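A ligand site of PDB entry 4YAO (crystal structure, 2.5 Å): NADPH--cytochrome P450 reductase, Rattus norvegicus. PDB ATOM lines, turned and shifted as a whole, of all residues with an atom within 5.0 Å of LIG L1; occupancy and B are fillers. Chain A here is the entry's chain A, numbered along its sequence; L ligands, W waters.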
ATOM      1  N   HIS A 262      28.787 -15.003  -7.258  1.00  0.00           N
ATOM      2  CA  HIS A 262      27.735 -15.773  -7.900  1.00  0.00           C
ATOM      3  C   HIS A 262      26.371 -15.281  -7.446  1.00  0.00           C
ATOM      4  O   HIS A 262      26.233 -14.740  -6.344  1.00  0.00           O
ATOM      5  CB  HIS A 262      27.882 -17.256  -7.583  1.00  0.00           C
ATOM      6  CG  HIS A 262      29.101 -17.885  -8.184  1.00  0.00           C
ATOM      7  ND1 HIS A 262      30.285 -18.026  -7.491  1.00  0.00           N
ATOM      8  CD2 HIS A 262      29.320 -18.420  -9.406  1.00  0.00           C
ATOM      9  CE1 HIS A 262      31.178 -18.611  -8.258  1.00  0.00           C
ATOM     10  NE2 HIS A 262      30.621 -18.861  -9.436  1.00  0.00           N
ATOM     11  N   THR A 321      12.803 -33.905 -11.270  1.00  0.00           N
ATOM     12  CA  THR A 321      13.430 -34.119 -12.568  1.00  0.00           C
ATOM     13  C   THR A 321      14.733 -34.895 -12.503  1.00  0.00           C
ATOM     14  O   THR A 321      15.157 -35.487 -13.496  1.00  0.00           O
ATOM     15  CB  THR A 321      13.745 -32.786 -13.241  1.00  0.00           C
ATOM     16  OG1 THR A 321      14.675 -32.072 -12.431  1.00  0.00           O
ATOM     17  CG2 THR A 321      12.479 -31.955 -13.428  1.00  0.00           C
ATOM     18  N   ASN A 322      15.393 -34.884 -11.360  1.00  0.00           N
ATOM     19  CA  ASN A 322      16.635 -35.630 -11.315  1.00  0.00           C
ATOM     20  C   ASN A 322      16.403 -37.093 -11.083  1.00  0.00           C
ATOM     21  O   ASN A 322      15.411 -37.493 -10.477  1.00  0.00           O
ATOM     22  CB  ASN A 322      17.574 -35.097 -10.243  1.00  0.00           C
ATOM     23  CG  ASN A 322      18.323 -33.882 -10.703  1.00  0.00           C
ATOM     24  OD1 ASN A 322      18.432 -33.636 -11.908  1.00  0.00           O
ATOM     25  ND2 ASN A 322      18.860 -33.108  -9.771  1.00  0.00           N
ATOM     26  N   ARG A 367      18.341 -41.235 -17.561  1.00  0.00           N
ATOM     27  CA  ARG A 367      17.919 -39.965 -16.981  1.00  0.00           C
ATOM     28  C   ARG A 367      16.400 -39.851 -16.810  1.00  0.00           C
ATOM     29  O   ARG A 367      15.814 -38.834 -17.141  1.00  0.00           O
ATOM     30  CB  ARG A 367      18.412 -38.783 -17.844  1.00  0.00           C
ATOM     31  CG  ARG A 367      19.937 -38.530 -17.829  1.00  0.00           C
ATOM     32  CD  ARG A 367      20.409 -37.900 -16.521  1.00  0.00           C
ATOM     33  NE  ARG A 367      19.633 -36.715 -16.175  1.00  0.00           N
ATOM     34  CZ  ARG A 367      19.748 -36.011 -15.059  1.00  0.00           C
ATOM     35  NH1 ARG A 367      18.972 -34.936 -14.864  1.00  0.00           N
ATOM     36  NH2 ARG A 367      20.620 -36.355 -14.120  1.00  0.00           N
ATOM     37  N   ARG A 397      19.973 -22.669  -8.214  1.00  0.00           N
ATOM     38  CA  ARG A 397      21.048 -22.755  -9.222  1.00  0.00           C
ATOM     39  C   ARG A 397      21.962 -21.513  -9.213  1.00  0.00           C
ATOM     40  O   ARG A 397      21.485 -20.382  -9.093  1.00  0.00           O
ATOM     41  CB  ARG A 397      20.468 -22.948 -10.628  1.00  0.00           C
ATOM     42  CG  ARG A 397      20.142 -24.378 -11.016  1.00  0.00           C
ATOM     43  CD  ARG A 397      19.000 -24.976 -10.201  1.00  0.00           C
ATOM     44  NE  ARG A 397      18.644 -26.296 -10.705  1.00  0.00           N
ATOM     45  CZ  ARG A 397      17.867 -27.167 -10.060  1.00  0.00           C
ATOM     46  NH1 ARG A 397      17.590 -28.349 -10.622  1.00  0.00           N
ATOM     47  NH2 ARG A 397      17.368 -26.881  -8.870  1.00  0.00           N
ATOM     48  N   TYR A 398      23.259 -21.737  -9.345  1.00  0.00           N
ATOM     49  CA  TYR A 398      24.266 -20.665  -9.360  1.00  0.00           C
ATOM     50  C   TYR A 398      24.665 -20.233 -10.747  1.00  0.00           C
ATOM     51  O   TYR A 398      24.647 -21.021 -11.691  1.00  0.00           O
ATOM     52  CB  TYR A 398      25.520 -21.112  -8.598  1.00  0.00           C
ATOM     53  CG  TYR A 398      25.311 -21.127  -7.118  1.00  0.00           C
ATOM     54  CD1 TYR A 398      25.254 -19.927  -6.413  1.00  0.00           C
ATOM     55  CD2 TYR A 398      25.069 -22.317  -6.425  1.00  0.00           C
ATOM     56  CE1 TYR A 398      24.966 -19.911  -5.057  1.00  0.00           C
ATOM     57  CE2 TYR A 398      24.763 -22.304  -5.055  1.00  0.00           C
ATOM     58  CZ  TYR A 398      24.712 -21.095  -4.385  1.00  0.00           C
ATOM     59  OH  TYR A 398      24.348 -21.029  -3.062  1.00  0.00           O
ATOM     60  N   TYR A 399      25.053 -18.965 -10.852  1.00  0.00           N
ATOM     61  CA  TYR A 399      25.470 -18.343 -12.109  1.00  0.00           C
ATOM     62  C   TYR A 399      26.513 -17.309 -11.750  1.00  0.00           C
ATOM     63  O   TYR A 399      26.376 -16.634 -10.715  1.00  0.00           O
ATOM     64  CB  TYR A 399      24.259 -17.681 -12.791  1.00  0.00           C
ATOM     65  CG  TYR A 399      23.228 -18.706 -13.170  1.00  0.00           C
ATOM     66  CD1 TYR A 399      23.402 -19.509 -14.294  1.00  0.00           C
ATOM     67  CD2 TYR A 399      22.151 -18.974 -12.351  1.00  0.00           C
ATOM     68  CE1 TYR A 399      22.550 -20.550 -14.588  1.00  0.00           C
ATOM     69  CE2 TYR A 399      21.275 -20.023 -12.633  1.00  0.00           C
ATOM     70  CZ  TYR A 399      21.491 -20.812 -13.759  1.00  0.00           C
ATOM     71  OH  TYR A 399      20.679 -21.906 -14.028  1.00  0.00           O
ATOM     72  N   SER A 400      27.547 -17.193 -12.569  1.00  0.00           N
ATOM     73  CA  SER A 400      28.626 -16.241 -12.334  1.00  0.00           C
ATOM     74  C   SER A 400      28.191 -14.847 -12.787  1.00  0.00           C
ATOM     75  O   SER A 400      28.168 -14.550 -13.986  1.00  0.00           O
ATOM     76  CB  SER A 400      29.863 -16.666 -13.104  1.00  0.00           C
ATOM     77  OG  SER A 400      30.076 -18.055 -13.009  1.00  0.00           O
ATOM     78  N   CYS A 415      24.738 -14.958 -17.593  1.00  0.00           N
ATOM     79  CA  CYS A 415      24.994 -15.472 -18.928  1.00  0.00           C
ATOM     80  C   CYS A 415      24.803 -16.971 -18.794  1.00  0.00           C
ATOM     81  O   CYS A 415      25.495 -17.582 -18.002  1.00  0.00           O
ATOM     82  CB  CYS A 415      26.415 -15.168 -19.365  1.00  0.00           C
ATOM     83  SG  CYS A 415      26.853 -15.898 -20.932  1.00  0.00           S
ATOM     84  N   ALA A 416      23.888 -17.549 -19.557  1.00  0.00           N
ATOM     85  CA  ALA A 416      23.627 -18.966 -19.436  1.00  0.00           C
ATOM     86  C   ALA A 416      23.092 -19.673 -20.691  1.00  0.00           C
ATOM     87  O   ALA A 416      22.560 -19.034 -21.609  1.00  0.00           O
ATOM     88  CB  ALA A 416      22.667 -19.195 -18.273  1.00  0.00           C
ATOM     89  N   VAL A 417      23.249 -20.998 -20.715  1.00  0.00           N
ATOM     90  CA  VAL A 417      22.760 -21.804 -21.812  1.00  0.00           C
ATOM     91  C   VAL A 417      21.570 -22.609 -21.271  1.00  0.00           C
ATOM     92  O   VAL A 417      21.621 -23.119 -20.157  1.00  0.00           O
ATOM     93  CB  VAL A 417      23.862 -22.759 -22.354  1.00  0.00           C
ATOM     94  CG1 VAL A 417      24.317 -23.743 -21.255  1.00  0.00           C
ATOM     95  CG2 VAL A 417      23.344 -23.509 -23.589  1.00  0.00           C
ATOM     96  N   VAL A 419      19.050 -25.711 -20.892  1.00  0.00           N
ATOM     97  CA  VAL A 419      19.187 -27.153 -20.993  1.00  0.00           C
ATOM     98  C   VAL A 419      17.913 -27.854 -21.463  1.00  0.00           C
ATOM     99  O   VAL A 419      16.839 -27.743 -20.864  1.00  0.00           O
ATOM    100  CB  VAL A 419      19.625 -27.761 -19.628  1.00  0.00           C
ATOM    101  CG1 VAL A 419      19.744 -29.268 -19.748  1.00  0.00           C
ATOM    102  CG2 VAL A 419      20.941 -27.171 -19.226  1.00  0.00           C
ATOM    103  N   TYR A 421      17.443 -31.634 -23.791  1.00  0.00           N
ATOM    104  CA  TYR A 421      18.090 -32.681 -24.578  1.00  0.00           C
ATOM    105  C   TYR A 421      17.205 -33.895 -24.659  1.00  0.00           C
ATOM    106  O   TYR A 421      16.247 -34.025 -23.899  1.00  0.00           O
ATOM    107  CB  TYR A 421      19.421 -33.082 -23.913  1.00  0.00           C
ATOM    108  CG  TYR A 421      19.289 -33.556 -22.465  1.00  0.00           C
ATOM    109  CD1 TYR A 421      19.052 -32.647 -21.428  1.00  0.00           C
ATOM    110  CD2 TYR A 421      19.342 -34.907 -22.141  1.00  0.00           C
ATOM    111  CE1 TYR A 421      18.865 -33.082 -20.117  1.00  0.00           C
ATOM    112  CE2 TYR A 421      19.164 -35.356 -20.821  1.00  0.00           C
ATOM    113  CZ  TYR A 421      18.917 -34.427 -19.806  1.00  0.00           C
ATOM    114  OH  TYR A 421      18.718 -34.861 -18.502  1.00  0.00           O
ATOM    115  N   LYS A 430      14.103 -31.076 -19.595  1.00  0.00           N
ATOM    116  CA  LYS A 430      14.392 -29.652 -19.584  1.00  0.00           C
ATOM    117  C   LYS A 430      14.978 -29.188 -18.251  1.00  0.00           C
ATOM    118  O   LYS A 430      14.511 -29.584 -17.185  1.00  0.00           O
ATOM    119  CB  LYS A 430      13.120 -28.858 -19.931  1.00  0.00           C
ATOM    120  CG  LYS A 430      12.593 -29.160 -21.327  1.00  0.00           C
ATOM    121  CD  LYS A 430      11.396 -28.296 -21.707  1.00  0.00           C
ATOM    122  CE  LYS A 430      11.073 -28.464 -23.194  1.00  0.00           C
ATOM    123  NZ  LYS A 430       9.930 -27.604 -23.635  1.00  0.00           N
ATOM    124  N   GLY A 431      16.015 -28.361 -18.318  1.00  0.00           N
ATOM    125  CA  GLY A 431      16.631 -27.849 -17.110  1.00  0.00           C
ATOM    126  C   GLY A 431      15.619 -27.041 -16.337  1.00  0.00           C
ATOM    127  O   GLY A 431      14.852 -26.268 -16.904  1.00  0.00           O
ATOM    128  N   VAL A 432      15.603 -27.234 -15.020  1.00  0.00           N
ATOM    129  CA  VAL A 432      14.655 -26.527 -14.173  1.00  0.00           C
ATOM    130  C   VAL A 432      14.870 -25.013 -14.179  1.00  0.00           C
ATOM    131  O   VAL A 432      13.960 -24.251 -14.484  1.00  0.00           O
ATOM    132  CB  VAL A 432      14.729 -27.044 -12.688  1.00  0.00           C
ATOM    133  CG1 VAL A 432      13.579 -26.449 -11.849  1.00  0.00           C
ATOM    134  CG2 VAL A 432      14.660 -28.571 -12.665  1.00  0.00           C
ATOM    135  N   ALA A 433      16.076 -24.582 -13.848  1.00  0.00           N
ATOM    136  CA  ALA A 433      16.354 -23.145 -13.763  1.00  0.00           C
ATOM    137  C   ALA A 433      16.336 -22.427 -15.097  1.00  0.00           C
ATOM    138  O   ALA A 433      15.738 -21.351 -15.237  1.00  0.00           O
ATOM    139  CB  ALA A 433      17.698 -22.893 -13.024  1.00  0.00           C
ATOM    140  N   THR A 434      17.008 -23.017 -16.088  1.00  0.00           N
ATOM    141  CA  THR A 434      17.103 -22.431 -17.407  1.00  0.00           C
ATOM    142  C   THR A 434      15.771 -22.308 -18.147  1.00  0.00           C
ATOM    143  O   THR A 434      15.458 -21.240 -18.662  1.00  0.00           O
ATOM    144  CB  THR A 434      18.053 -23.232 -18.254  1.00  0.00           C
ATOM    145  OG1 THR A 434      17.495 -24.535 -18.477  1.00  0.00           O
ATOM    146  CG2 THR A 434      19.404 -23.363 -17.548  1.00  0.00           C
ATOM    147  N   SER A 435      14.988 -23.383 -18.202  1.00  0.00           N
ATOM    148  CA  SER A 435      13.688 -23.331 -18.894  1.00  0.00           C
ATOM    149  C   SER A 435      12.810 -22.281 -18.244  1.00  0.00           C
ATOM    150  O   SER A 435      11.927 -21.679 -18.873  1.00  0.00           O
ATOM    151  CB  SER A 435      12.942 -24.670 -18.781  1.00  0.00           C
ATOM    152  OG  SER A 435      13.720 -25.784 -19.191  1.00  0.00           O
ATOM    153  N   THR A 478      29.936 -20.424 -22.133  1.00  0.00           N
ATOM    154  CA  THR A 478      29.372 -19.626 -21.035  1.00  0.00           C
ATOM    155  C   THR A 478      30.424 -19.123 -20.043  1.00  0.00           C
ATOM    156  O   THR A 478      30.155 -18.191 -19.278  1.00  0.00           O
ATOM    157  CB  THR A 478      28.291 -20.386 -20.216  1.00  0.00           C
ATOM    158  OG1 THR A 478      28.672 -21.747 -20.040  1.00  0.00           O
ATOM    159  CG2 THR A 478      26.935 -20.293 -20.892  1.00  0.00           C
ATOM    160  N   ALA A 481      31.090 -15.184 -18.870  1.00  0.00           N
ATOM    161  CA  ALA A 481      30.271 -14.243 -18.111  1.00  0.00           C
ATOM    162  C   ALA A 481      30.976 -13.529 -16.959  1.00  0.00           C
ATOM    163  O   ALA A 481      30.757 -12.328 -16.764  1.00  0.00           O
ATOM    164  CB  ALA A 481      29.010 -14.934 -17.616  1.00  0.00           C
ATOM    165  N   ASP A 618      36.940 -21.153 -11.746  1.00  0.00           N
ATOM    166  CA  ASP A 618      35.510 -20.992 -11.593  1.00  0.00           C
ATOM    167  C   ASP A 618      34.906 -21.909 -12.636  1.00  0.00           C
ATOM    168  O   ASP A 618      34.207 -21.483 -13.565  1.00  0.00           O
ATOM    169  CB  ASP A 618      35.083 -19.543 -11.818  1.00  0.00           C
ATOM    170  CG  ASP A 618      33.584 -19.345 -11.643  1.00  0.00           C
ATOM    171  OD1 ASP A 618      33.005 -19.937 -10.702  1.00  0.00           O
ATOM    172  OD2 ASP A 618      32.974 -18.589 -12.446  1.00  0.00           O
ATOM    173  N   TRP A 620      32.697 -25.447 -13.591  1.00  0.00           N
ATOM    174  CA  TRP A 620      31.555 -26.194 -13.096  1.00  0.00           C
ATOM    175  C   TRP A 620      31.242 -27.288 -14.080  1.00  0.00           C
ATOM    176  O   TRP A 620      31.504 -27.143 -15.264  1.00  0.00           O
ATOM    177  CB  TRP A 620      30.372 -25.259 -12.928  1.00  0.00           C
ATOM    178  CG  TRP A 620      29.875 -24.680 -14.213  1.00  0.00           C
ATOM    179  CD1 TRP A 620      29.027 -25.267 -15.100  1.00  0.00           C
ATOM    180  CD2 TRP A 620      30.156 -23.370 -14.735  1.00  0.00           C
ATOM    181  NE1 TRP A 620      28.748 -24.411 -16.136  1.00  0.00           N
ATOM    182  CE2 TRP A 620      29.429 -23.234 -15.941  1.00  0.00           C
ATOM    183  CE3 TRP A 620      30.945 -22.304 -14.295  1.00  0.00           C
ATOM    184  CZ2 TRP A 620      29.471 -22.081 -16.718  1.00  0.00           C
ATOM    185  CZ3 TRP A 620      30.994 -21.145 -15.070  1.00  0.00           C
ATOM    186  CH2 TRP A 620      30.251 -21.041 -16.265  1.00  0.00           C
HETATM  187  P1  LIG L   1      19.051 -29.054 -14.166  1.00  0.00           P
HETATM  188  O1  LIG L   1      17.626 -29.442 -14.006  1.00  0.00           O
HETATM  189  O2  LIG L   1      19.859 -28.748 -12.972  1.00  0.00           O
HETATM  190  O3  LIG L   1      19.777 -30.241 -14.978  1.00  0.00           O
HETATM  191  C1  LIG L   1      21.203 -30.279 -15.081  1.00  0.00           C
HETATM  192  C2  LIG L   1      21.606 -31.704 -15.457  1.00  0.00           C
HETATM  193  O4  LIG L   1      21.006 -32.114 -16.692  1.00  0.00           O
HETATM  194  C3  LIG L   1      23.087 -31.781 -15.766  1.00  0.00           C
HETATM  195  O5  LIG L   1      23.823 -31.740 -14.527  1.00  0.00           O
HETATM  196  C4  LIG L   1      23.082 -33.188 -16.326  1.00  0.00           C
HETATM  197  O6  LIG L   1      22.889 -34.136 -15.261  1.00  0.00           O
HETATM  198  C5  LIG L   1      21.849 -33.147 -17.213  1.00  0.00           C
HETATM  199  N1  LIG L   1      22.181 -32.762 -18.605  1.00  0.00           N
HETATM  200  C6  LIG L   1      22.421 -31.390 -19.095  1.00  0.00           C
HETATM  201  N2  LIG L   1      22.439 -31.637 -20.552  1.00  0.00           N
HETATM  202  C7  LIG L   1      22.403 -32.957 -20.749  1.00  0.00           C
HETATM  203  C8  LIG L   1      22.391 -33.638 -21.894  1.00  0.00           C
HETATM  204  N3  LIG L   1      22.347 -32.919 -23.007  1.00  0.00           N
HETATM  205  N4  LIG L   1      22.509 -34.974 -21.937  1.00  0.00           N
HETATM  206  C9  LIG L   1      22.668 -35.675 -20.725  1.00  0.00           C
HETATM  207  N5  LIG L   1      22.665 -34.928 -19.547  1.00  0.00           N
HETATM  208  C10 LIG L   1      22.518 -33.592 -19.579  1.00  0.00           C
HETATM  209  N6  LIG L   1      25.757 -22.026 -15.937  1.00  0.00           N
HETATM  210  C11 LIG L   1      25.732 -20.919 -16.801  1.00  0.00           C
HETATM  211  O7  LIG L   1      25.212 -21.019 -17.911  1.00  0.00           O
HETATM  212  N7  LIG L   1      26.405 -19.746 -16.456  1.00  0.00           N
HETATM  213  C12 LIG L   1      27.114 -19.677 -15.251  1.00  0.00           C
HETATM  214  O8  LIG L   1      27.457 -18.570 -14.834  1.00  0.00           O
HETATM  215  C13 LIG L   1      27.151 -20.774 -14.405  1.00  0.00           C
HETATM  216  N8  LIG L   1      27.971 -20.787 -13.340  1.00  0.00           N
HETATM  217  C14 LIG L   1      27.981 -21.832 -12.511  1.00  0.00           C
HETATM  218  C15 LIG L   1      28.752 -21.794 -11.358  1.00  0.00           C
HETATM  219  C16 LIG L   1      28.658 -22.804 -10.409  1.00  0.00           C
HETATM  220  C17 LIG L   1      29.242 -22.628  -9.161  1.00  0.00           C
HETATM  221  C18 LIG L   1      27.816 -23.881 -10.640  1.00  0.00           C
HETATM  222  C19 LIG L   1      27.769 -24.941  -9.734  1.00  0.00           C
HETATM  223  C20 LIG L   1      27.053 -23.937 -11.809  1.00  0.00           C
HETATM  224  C21 LIG L   1      27.122 -22.911 -12.729  1.00  0.00           C
HETATM  225  N9  LIG L   1      26.343 -22.917 -13.824  1.00  0.00           N
HETATM  226  C22 LIG L   1      26.473 -21.944 -14.742  1.00  0.00           C
HETATM  227  C23 LIG L   1      25.419 -24.044 -14.091  1.00  0.00           C
HETATM  228  C24 LIG L   1      24.045 -23.773 -13.482  1.00  0.00           C
HETATM  229  O9  LIG L   1      24.159 -23.590 -12.074  1.00  0.00           O
HETATM  230  C25 LIG L   1      23.086 -24.927 -13.776  1.00  0.00           C
HETATM  231  O10 LIG L   1      23.758 -26.164 -13.519  1.00  0.00           O
HETATM  232  C26 LIG L   1      22.632 -24.880 -15.238  1.00  0.00           C
HETATM  233  O11 LIG L   1      22.100 -23.574 -15.513  1.00  0.00           O
HETATM  234  C27 LIG L   1      21.567 -25.947 -15.496  1.00  0.00           C
HETATM  235  O12 LIG L   1      20.574 -25.865 -14.475  1.00  0.00           O
HETATM  236  P2  LIG L   1      19.035 -26.287 -14.719  1.00  0.00           P
HETATM  237  O13 LIG L   1      18.495 -25.505 -15.853  1.00  0.00           O
HETATM  238  O14 LIG L   1      18.350 -26.200 -13.412  1.00  0.00           O
HETATM  239  O15 LIG L   1      19.142 -27.823 -15.194  1.00  0.00           O
HETATM  240  N1  LG2 L   2      34.615 -31.848  -4.617  1.00  0.00           N
HETATM  241  C1  LG2 L   2      35.832 -32.127  -4.131  1.00  0.00           C
HETATM  242  O1  LG2 L   2      36.171 -33.288  -3.875  1.00  0.00           O
HETATM  243  N2  LG2 L   2      36.687 -31.070  -3.923  1.00  0.00           N
HETATM  244  C2  LG2 L   2      36.428 -29.718  -4.179  1.00  0.00           C
HETATM  245  O2  LG2 L   2      37.361 -28.971  -3.920  1.00  0.00           O
HETATM  246  C3  LG2 L   2      35.142 -29.406  -4.713  1.00  0.00           C
HETATM  247  N3  LG2 L   2      34.857 -28.062  -4.994  1.00  0.00           N
HETATM  248  C4  LG2 L   2      33.580 -27.843  -5.512  1.00  0.00           C
HETATM  249  C5  LG2 L   2      33.285 -26.479  -5.816  1.00  0.00           C
HETATM  250  C6  LG2 L   2      32.038 -26.110  -6.365  1.00  0.00           C
HETATM  251  C7  LG2 L   2      31.848 -24.593  -6.645  1.00  0.00           C
HETATM  252  C8  LG2 L   2      30.985 -27.137  -6.638  1.00  0.00           C
HETATM  253  C9  LG2 L   2      29.739 -26.903  -7.165  1.00  0.00           C
HETATM  254  C10 LG2 L   2      31.262 -28.464  -6.341  1.00  0.00           C
HETATM  255  C11 LG2 L   2      32.556 -28.874  -5.779  1.00  0.00           C
HETATM  256  N4  LG2 L   2      32.936 -30.264  -5.454  1.00  0.00           N
HETATM  257  C12 LG2 L   2      34.276 -30.538  -4.897  1.00  0.00           C
HETATM  258  C13 LG2 L   2      32.012 -31.382  -5.665  1.00  0.00           C
HETATM  259  C14 LG2 L   2      31.099 -31.704  -4.440  1.00  0.00           C
HETATM  260  O3  LG2 L   2      31.959 -31.999  -3.283  1.00  0.00           O
HETATM  261  C15 LG2 L   2      30.179 -32.900  -4.735  1.00  0.00           C
HETATM  262  O4  LG2 L   2      29.361 -32.537  -5.872  1.00  0.00           O
HETATM  263  C16 LG2 L   2      29.313 -33.177  -3.446  1.00  0.00           C
HETATM  264  O5  LG2 L   2      28.547 -34.352  -3.870  1.00  0.00           O
HETATM  265  C17 LG2 L   2      28.287 -32.107  -3.124  1.00  0.00           C
HETATM  266  O6  LG2 L   2      27.577 -32.421  -1.865  1.00  0.00           O
HETATM  267  P1  LG2 L   2      26.436 -31.575  -1.176  1.00  0.00           P
HETATM  268  O7  LG2 L   2      25.194 -31.621  -1.976  1.00  0.00           O
HETATM  269  O8  LG2 L   2      27.143 -30.220  -0.878  1.00  0.00           O
HETATM  270  O9  LG2 L   2      26.182 -32.432   0.140  1.00  0.00           O
HETATM  271  O   HOH W   1      25.704 -33.514 -12.897  1.00  0.00           O
HETATM  272  O   HOH W   2      23.347 -24.770  -9.396  1.00  0.00           O
HETATM  273  O   HOH W   3      26.173 -15.682 -15.425  1.00  0.00           O
HETATM  274  O   HOH W   4      21.984 -27.745 -12.065  1.00  0.00           O
HETATM  275  O   HOH W   5      16.305 -31.765 -15.803  1.00  0.00           O
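The backbone NH (N) of Tyr 398 lies within hydrogen-bond range of an oxygen (O9) of LIG L1. The backbone carbonyl oxygen (O) of Tyr 398 sits at hydrogen-bond distance from an oxygen (O9) of LIG L1, 2.6 Å away. The side-chain hydroxyl (OH) of Tyr 399 lies within hydrogen-bond range of an oxygen (O11) of LIG L1 (2.6 Å). An oxygen (O8) of LIG L1 sits at hydrogen-bond distance from the backbone NH of Ser 400, 2.7 Å away. The side-chain hydroxyl (OG) of Ser 400 lies within hydrogen-bond range of an oxygen (O8) of LIG L1, at 3.2 Å. The guanidinium group (NE) of Arg 397 lies within salt-bridge range of an oxygen (O14) of LIG L1, 2.7 Å away. N7 of LIG L1 is in hydrogen-bond range of O of Cys 415, at 2.8 Å. O14 of LIG L1 sits at hydrogen-bond distance from N of Ala 433 (2.8 Å). N of Thr 434 sits close to O13 of LIG L1, at 2.9 Å. The side-chain hydroxyl (OG1) of Thr 434 lies close to an oxygen (O13) of LIG L1. N of Val 432 sits at hydrogen-bond distance from O1 of LIG L1. NH2 of Arg 367 is in hydrogen-bond range of O6 of LIG L1, 3.4 Å away. The backbone NH of Val 417 lies within hydrogen-bond range of an oxygen (O7) of LIG L1.
His 262 touches LIG L1 (CD2 to C15, 3.9 Å). CA of Ala 416 touches O7 of LIG L1, 3.0 Å away. Val 419 touches LIG L1. CB of Tyr 421 touches N3 of LIG L1 (3.1 Å). CA of Gly 431 touches O15 of LIG L1, at 3.2 Å. Thr 478 touches LIG L1. CE2 of Trp 620 touches C22 of LIG L1, 3.4 Å away. Hydrophobic or aromatic side chains that line LIG L1: His 262, Tyr 398, Tyr 399, Ala 416, Val 419, Tyr 421, Val 432, Ala 433 and Trp 620. 17 residues have an atom within 4 Å of LIG L1: His 262, Arg 367, Arg 397, Tyr 398, Tyr 399, Ser 400, Cys 415, Ala 416, Val 417, Val 419, Tyr 421, Gly 431, Val 432, Ala 433, Thr 434, Thr 478 and Trp 620. Along chain A the residues within 4 Å of LIG L1 span positions 262 to 620.
Water W2 lies within hydrogen-bond range of N of Tyr 398 (3.0 Å) and O9 of LIG L1 (3.0 Å). Water W3 lies within hydrogen-bond range of N of Cys 415 (2.7 Å), O of Ser 400 (2.7 Å) and O8 of LIG L1 (3.2 Å). Water W5 lies within hydrogen-bond range of the backbone carbonyl oxygen of Lys 430 and an oxygen (O1) of LIG L1.
OG of Ser 400 lies within hydrogen-bond range of OD2 of Asp 618 (3.0 Å). The side-chain hydroxyl (OG1) of Thr 434 sits at hydrogen-bond distance from the backbone NH (N) of Val 419 (3.1 Å). The side-chain hydroxyl of Tyr 421 is in hydrogen-bond range of the guanidinium group of Arg 367. The backbone NH of Gly 431 sits at hydrogen-bond distance from the backbone carbonyl oxygen of Val 419 (2.7 Å). O of Gly 431 lies within hydrogen-bond range of OG of Ser 435 (2.6 Å). NH1 of Arg 367 lies within hydrogen-bond range of OD1 of Asn 322, at 3.3 Å. OD1 of Asp 618 sits at hydrogen-bond distance from NE2 of His 262 (2.9 Å).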
